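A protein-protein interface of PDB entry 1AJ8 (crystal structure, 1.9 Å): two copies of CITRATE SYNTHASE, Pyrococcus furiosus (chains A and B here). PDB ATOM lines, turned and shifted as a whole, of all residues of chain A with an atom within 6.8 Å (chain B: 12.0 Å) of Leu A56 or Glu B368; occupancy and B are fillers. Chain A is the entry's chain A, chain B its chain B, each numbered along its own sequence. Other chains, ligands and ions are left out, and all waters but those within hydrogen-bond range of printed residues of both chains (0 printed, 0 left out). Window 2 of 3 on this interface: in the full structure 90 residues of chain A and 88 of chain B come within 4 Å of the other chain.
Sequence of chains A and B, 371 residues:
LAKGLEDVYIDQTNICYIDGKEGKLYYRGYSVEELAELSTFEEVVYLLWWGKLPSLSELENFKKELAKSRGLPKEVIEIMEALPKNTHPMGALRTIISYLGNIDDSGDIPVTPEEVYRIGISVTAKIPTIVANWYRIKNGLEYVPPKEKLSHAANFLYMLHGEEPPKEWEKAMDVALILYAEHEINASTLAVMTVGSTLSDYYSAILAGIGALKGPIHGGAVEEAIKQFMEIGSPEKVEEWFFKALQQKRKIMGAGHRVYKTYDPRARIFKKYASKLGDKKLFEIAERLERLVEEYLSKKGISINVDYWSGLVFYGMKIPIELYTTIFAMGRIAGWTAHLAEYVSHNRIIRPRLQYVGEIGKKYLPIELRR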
ATOM      1  N   PRO A  54       2.567  23.023 -31.574  1.00  0.00           N
ATOM      2  CA  PRO A  54       2.410  24.424 -31.966  1.00  0.00           C
ATOM      3  C   PRO A  54       3.217  25.411 -31.137  1.00  0.00           C
ATOM      4  O   PRO A  54       3.612  25.129 -30.005  1.00  0.00           O
ATOM      5  CB  PRO A  54       0.914  24.667 -31.818  1.00  0.00           C
ATOM      6  CG  PRO A  54       0.511  23.736 -30.723  1.00  0.00           C
ATOM      7  CD  PRO A  54       1.394  22.521 -30.839  1.00  0.00           C
ATOM      8  N   SER A  55       3.468  26.570 -31.724  1.00  0.00           N
ATOM      9  CA  SER A  55       4.184  27.624 -31.033  1.00  0.00           C
ATOM     10  C   SER A  55       3.114  28.304 -30.198  1.00  0.00           C
ATOM     11  O   SER A  55       1.932  27.983 -30.318  1.00  0.00           O
ATOM     12  CB  SER A  55       4.765  28.622 -32.034  1.00  0.00           C
ATOM     13  OG  SER A  55       3.743  29.438 -32.582  1.00  0.00           O
ATOM     14  N   LEU A  56       3.522  29.244 -29.359  1.00  0.00           N
ATOM     15  CA  LEU A  56       2.573  29.958 -28.518  1.00  0.00           C
ATOM     16  C   LEU A  56       1.429  30.541 -29.351  1.00  0.00           C
ATOM     17  O   LEU A  56       0.255  30.320 -29.056  1.00  0.00           O
ATOM     18  CB  LEU A  56       3.291  31.088 -27.767  1.00  0.00           C
ATOM     19  CG  LEU A  56       3.163  31.204 -26.243  1.00  0.00           C
ATOM     20  CD1 LEU A  56       1.851  30.604 -25.755  1.00  0.00           C
ATOM     21  CD2 LEU A  56       4.342  30.506 -25.599  1.00  0.00           C
ATOM     22  N   SER A  57       1.783  31.277 -30.399  1.00  0.00           N
ATOM     23  CA  SER A  57       0.792  31.918 -31.254  1.00  0.00           C
ATOM     24  C   SER A  57       0.003  30.950 -32.116  1.00  0.00           C
ATOM     25  O   SER A  57      -1.171  31.184 -32.395  1.00  0.00           O
ATOM     26  CB  SER A  57       1.466  32.964 -32.147  1.00  0.00           C
ATOM     27  OG  SER A  57       2.367  32.358 -33.056  1.00  0.00           O
ATOM     28  N   GLU A  58       0.646  29.871 -32.550  1.00  0.00           N
ATOM     29  CA  GLU A  58      -0.025  28.881 -33.382  1.00  0.00           C
ATOM     30  C   GLU A  58      -1.143  28.227 -32.592  1.00  0.00           C
ATOM     31  O   GLU A  58      -2.244  28.031 -33.102  1.00  0.00           O
ATOM     32  CB  GLU A  58       0.965  27.821 -33.858  1.00  0.00           C
ATOM     33  CG  GLU A  58       1.737  28.249 -35.085  1.00  0.00           C
ATOM     34  CD  GLU A  58       2.876  27.312 -35.419  1.00  0.00           C
ATOM     35  OE1 GLU A  58       3.332  26.578 -34.517  1.00  0.00           O
ATOM     36  OE2 GLU A  58       3.315  27.309 -36.590  1.00  0.00           O
ATOM     37  N   LEU A  59      -0.856  27.903 -31.337  1.00  0.00           N
ATOM     38  CA  LEU A  59      -1.849  27.273 -30.482  1.00  0.00           C
ATOM     39  C   LEU A  59      -2.995  28.226 -30.129  1.00  0.00           C
ATOM     40  O   LEU A  59      -4.165  27.844 -30.195  1.00  0.00           O
ATOM     41  CB  LEU A  59      -1.191  26.756 -29.202  1.00  0.00           C
ATOM     42  CG  LEU A  59      -2.147  26.052 -28.237  1.00  0.00           C
ATOM     43  CD1 LEU A  59      -2.850  24.904 -28.947  1.00  0.00           C
ATOM     44  CD2 LEU A  59      -1.370  25.547 -27.031  1.00  0.00           C
ATOM     45  N   GLU A  60      -2.662  29.462 -29.763  1.00  0.00           N
ATOM     46  CA  GLU A  60      -3.682  30.444 -29.398  1.00  0.00           C
ATOM     47  C   GLU A  60      -4.620  30.711 -30.559  1.00  0.00           C
ATOM     48  O   GLU A  60      -5.828  30.821 -30.381  1.00  0.00           O
ATOM     49  CB  GLU A  60      -3.037  31.767 -28.964  1.00  0.00           C
ATOM     50  CG  GLU A  60      -3.247  32.127 -27.487  1.00  0.00           C
ATOM     51  CD  GLU A  60      -4.627  31.749 -26.956  1.00  0.00           C
ATOM     52  OE1 GLU A  60      -5.626  32.344 -27.416  1.00  0.00           O
ATOM     53  OE2 GLU A  60      -4.712  30.857 -26.079  1.00  0.00           O
ATOM     54  N   ASN A  61      -4.056  30.814 -31.754  1.00  0.00           N
ATOM     55  CA  ASN A  61      -4.861  31.071 -32.934  1.00  0.00           C
ATOM     56  C   ASN A  61      -5.737  29.875 -33.305  1.00  0.00           C
ATOM     57  O   ASN A  61      -6.875  30.046 -33.743  1.00  0.00           O
ATOM     58  CB  ASN A  61      -3.960  31.441 -34.107  1.00  0.00           C
ATOM     59  CG  ASN A  61      -4.715  31.484 -35.415  1.00  0.00           C
ATOM     60  OD1 ASN A  61      -4.825  30.475 -36.118  1.00  0.00           O
ATOM     61  ND2 ASN A  61      -5.252  32.656 -35.751  1.00  0.00           N
ATOM     62  N   LYS B 363      10.711  13.956 -27.312  1.00  0.00           N
ATOM     63  CA  LYS B 363      10.494  14.529 -25.993  1.00  0.00           C
ATOM     64  C   LYS B 363       9.716  15.835 -26.058  1.00  0.00           C
ATOM     65  O   LYS B 363      10.072  16.757 -26.790  1.00  0.00           O
ATOM     66  CB  LYS B 363      11.834  14.735 -25.286  1.00  0.00           C
ATOM     67  CG  LYS B 363      12.402  13.447 -24.686  1.00  0.00           C
ATOM     68  CD  LYS B 363      11.432  12.816 -23.676  1.00  0.00           C
ATOM     69  CE  LYS B 363      11.301  11.306 -23.876  1.00  0.00           C
ATOM     70  NZ  LYS B 363      10.256  10.705 -22.987  1.00  0.00           N
ATOM     71  N   TYR B 364       8.635  15.895 -25.289  1.00  0.00           N
ATOM     72  CA  TYR B 364       7.769  17.064 -25.235  1.00  0.00           C
ATOM     73  C   TYR B 364       8.518  18.315 -24.786  1.00  0.00           C
ATOM     74  O   TYR B 364       9.153  18.322 -23.731  1.00  0.00           O
ATOM     75  CB  TYR B 364       6.612  16.793 -24.273  1.00  0.00           C
ATOM     76  CG  TYR B 364       5.600  17.910 -24.198  1.00  0.00           C
ATOM     77  CD1 TYR B 364       5.816  19.019 -23.382  1.00  0.00           C
ATOM     78  CD2 TYR B 364       4.424  17.857 -24.942  1.00  0.00           C
ATOM     79  CE1 TYR B 364       4.884  20.053 -23.313  1.00  0.00           C
ATOM     80  CE2 TYR B 364       3.486  18.881 -24.881  1.00  0.00           C
ATOM     81  CZ  TYR B 364       3.721  19.978 -24.065  1.00  0.00           C
ATOM     82  OH  TYR B 364       2.799  21.003 -24.018  1.00  0.00           O
ATOM     83  N   LEU B 365       8.436  19.374 -25.584  1.00  0.00           N
ATOM     84  CA  LEU B 365       9.100  20.625 -25.244  1.00  0.00           C
ATOM     85  C   LEU B 365       8.073  21.675 -24.843  1.00  0.00           C
ATOM     86  O   LEU B 365       7.107  21.921 -25.569  1.00  0.00           O
ATOM     87  CB  LEU B 365       9.919  21.141 -26.431  1.00  0.00           C
ATOM     88  CG  LEU B 365      10.763  22.396 -26.173  1.00  0.00           C
ATOM     89  CD1 LEU B 365      12.025  22.021 -25.407  1.00  0.00           C
ATOM     90  CD2 LEU B 365      11.115  23.055 -27.495  1.00  0.00           C
ATOM     91  N   PRO B 366       8.255  22.288 -23.662  1.00  0.00           N
ATOM     92  CA  PRO B 366       7.333  23.318 -23.178  1.00  0.00           C
ATOM     93  C   PRO B 366       7.068  24.344 -24.274  1.00  0.00           C
ATOM     94  O   PRO B 366       7.990  24.767 -24.969  1.00  0.00           O
ATOM     95  CB  PRO B 366       8.066  23.916 -21.981  1.00  0.00           C
ATOM     96  CG  PRO B 366       8.903  22.795 -21.474  1.00  0.00           C
ATOM     97  CD  PRO B 366       9.338  22.027 -22.696  1.00  0.00           C
ATOM     98  N   ILE B 367       5.808  24.740 -24.419  1.00  0.00           N
ATOM     99  CA  ILE B 367       5.417  25.692 -25.449  1.00  0.00           C
ATOM    100  C   ILE B 367       6.244  26.981 -25.485  1.00  0.00           C
ATOM    101  O   ILE B 367       6.509  27.517 -26.561  1.00  0.00           O
ATOM    102  CB  ILE B 367       3.911  26.039 -25.325  1.00  0.00           C
ATOM    103  CG1 ILE B 367       3.435  26.754 -26.590  1.00  0.00           C
ATOM    104  CG2 ILE B 367       3.666  26.879 -24.092  1.00  0.00           C
ATOM    105  CD1 ILE B 367       2.001  26.451 -26.953  1.00  0.00           C
ATOM    106  N   GLU B 368       6.660  27.477 -24.323  1.00  0.00           N
ATOM    107  CA  GLU B 368       7.453  28.707 -24.278  1.00  0.00           C
ATOM    108  C   GLU B 368       8.836  28.492 -24.882  1.00  0.00           C
ATOM    109  O   GLU B 368       9.440  29.427 -25.415  1.00  0.00           O
ATOM    110  CB  GLU B 368       7.600  29.201 -22.839  1.00  0.00           C
ATOM    111  CG  GLU B 368       7.850  28.094 -21.832  1.00  0.00           C
ATOM    112  CD  GLU B 368       6.568  27.410 -21.410  1.00  0.00           C
ATOM    113  OE1 GLU B 368       5.515  28.088 -21.381  1.00  0.00           O
ATOM    114  OE2 GLU B 368       6.610  26.198 -21.109  1.00  0.00           O
ATOM    115  N   LEU B 369       9.333  27.259 -24.797  1.00  0.00           N
ATOM    116  CA  LEU B 369      10.646  26.912 -25.330  1.00  0.00           C
ATOM    117  C   LEU B 369      10.594  26.608 -26.827  1.00  0.00           C
ATOM    118  O   LEU B 369      11.612  26.274 -27.434  1.00  0.00           O
ATOM    119  CB  LEU B 369      11.215  25.702 -24.588  1.00  0.00           C
ATOM    120  CG  LEU B 369      11.598  25.918 -23.122  1.00  0.00           C
ATOM    121  CD1 LEU B 369      12.036  24.601 -22.495  1.00  0.00           C
ATOM    122  CD2 LEU B 369      12.711  26.940 -23.042  1.00  0.00           C
ATOM    123  N   ARG B 370       9.407  26.715 -27.416  1.00  0.00           N
ATOM    124  CA  ARG B 370       9.234  26.457 -28.843  1.00  0.00           C
ATOM    125  C   ARG B 370       9.399  27.770 -29.602  1.00  0.00           C
ATOM    126  O   ARG B 370       9.691  27.726 -30.820  1.00  0.00           O
ATOM    127  CB  ARG B 370       7.839  25.886 -29.123  1.00  0.00           C
ATOM    128  CG  ARG B 370       7.663  24.427 -28.746  1.00  0.00           C
ATOM    129  CD  ARG B 370       6.191  24.043 -28.761  1.00  0.00           C
ATOM    130  NE  ARG B 370       5.852  23.130 -27.674  1.00  0.00           N
ATOM    131  CZ  ARG B 370       4.610  22.873 -27.276  1.00  0.00           C
ATOM    132  NH1 ARG B 370       3.583  23.462 -27.876  1.00  0.00           N
ATOM    133  NH2 ARG B 370       4.397  22.038 -26.270  1.00  0.00           N
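Among the printed residues, pairs that only touch across the chains: Leu A59 with Ile B367 (3.5 Å), Pro A54 with Ile B367 (3.7 Å), Ser A55 with Ile B367 (3.7 Å), Leu A56 with Ile B367 (3.7 Å) and Leu A56 with Glu B368 (3.8 Å).
Of the 8 printed residues of chain B, 3 touch a printed residue of chain A.
Hydrophobic or aromatic side chains of chain B within 4 Å of the printed part of chain A: Ile B367.
Of the 8 printed residues of chain A, 4 touch a printed residue of chain B.
Among the printed residues, no Asp or Glu carboxylate lies within 4 Å of a Lys or Arg side-chain nitrogen of the other chain.
The backbone carbonyl oxygen (O) of Pro A54 is in hydrogen-bond range of the guanidinium group (NH1) of Arg B370 (2.7 Å).
Pro A54 touches just these residues of chain B: Ile B367 and Arg B370.
Of chain B, only Ile B367 and Glu B368 come within 4 Å of Leu A56.
Ser A57 touches none of the printed residues of chain B.
No residue of chain B comes within 4 Å of Glu A58.
Leu A59 touches just one residue of chain B: Ile B367.
Lys B363 touches none of the printed residues of chain A.
Of the printed residues of chain A, Ile B367 touches Pro A54, Ser A55, Leu A56 and Leu A59.
Of chain A, only Leu A56 comes within 4 Å of Glu B368.
Of the printed residues of chain A, Arg B370 touches Pro A54 (2.7 Å).
The nearest printed residue of chain A that does not touch Ile B367 is Ser A57 (5.9 Å).
No position is printed for both chains.
The guanidinium group of Arg B370 lies within hydrogen-bond range of the backbone carbonyl oxygen of Leu B365 (2.7 Å).
OE1 of Glu A58 is in hydrogen-bond range of N of Ser A55.
The side-chain hydroxyl (OG) of Ser A55 lies within hydrogen-bond range of the side-chain hydroxyl (OG) of Ser A57 (3.3 Å).
OH of Tyr B364 sits at hydrogen-bond distance from NH2 of Arg B370, at 2.9 Å.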
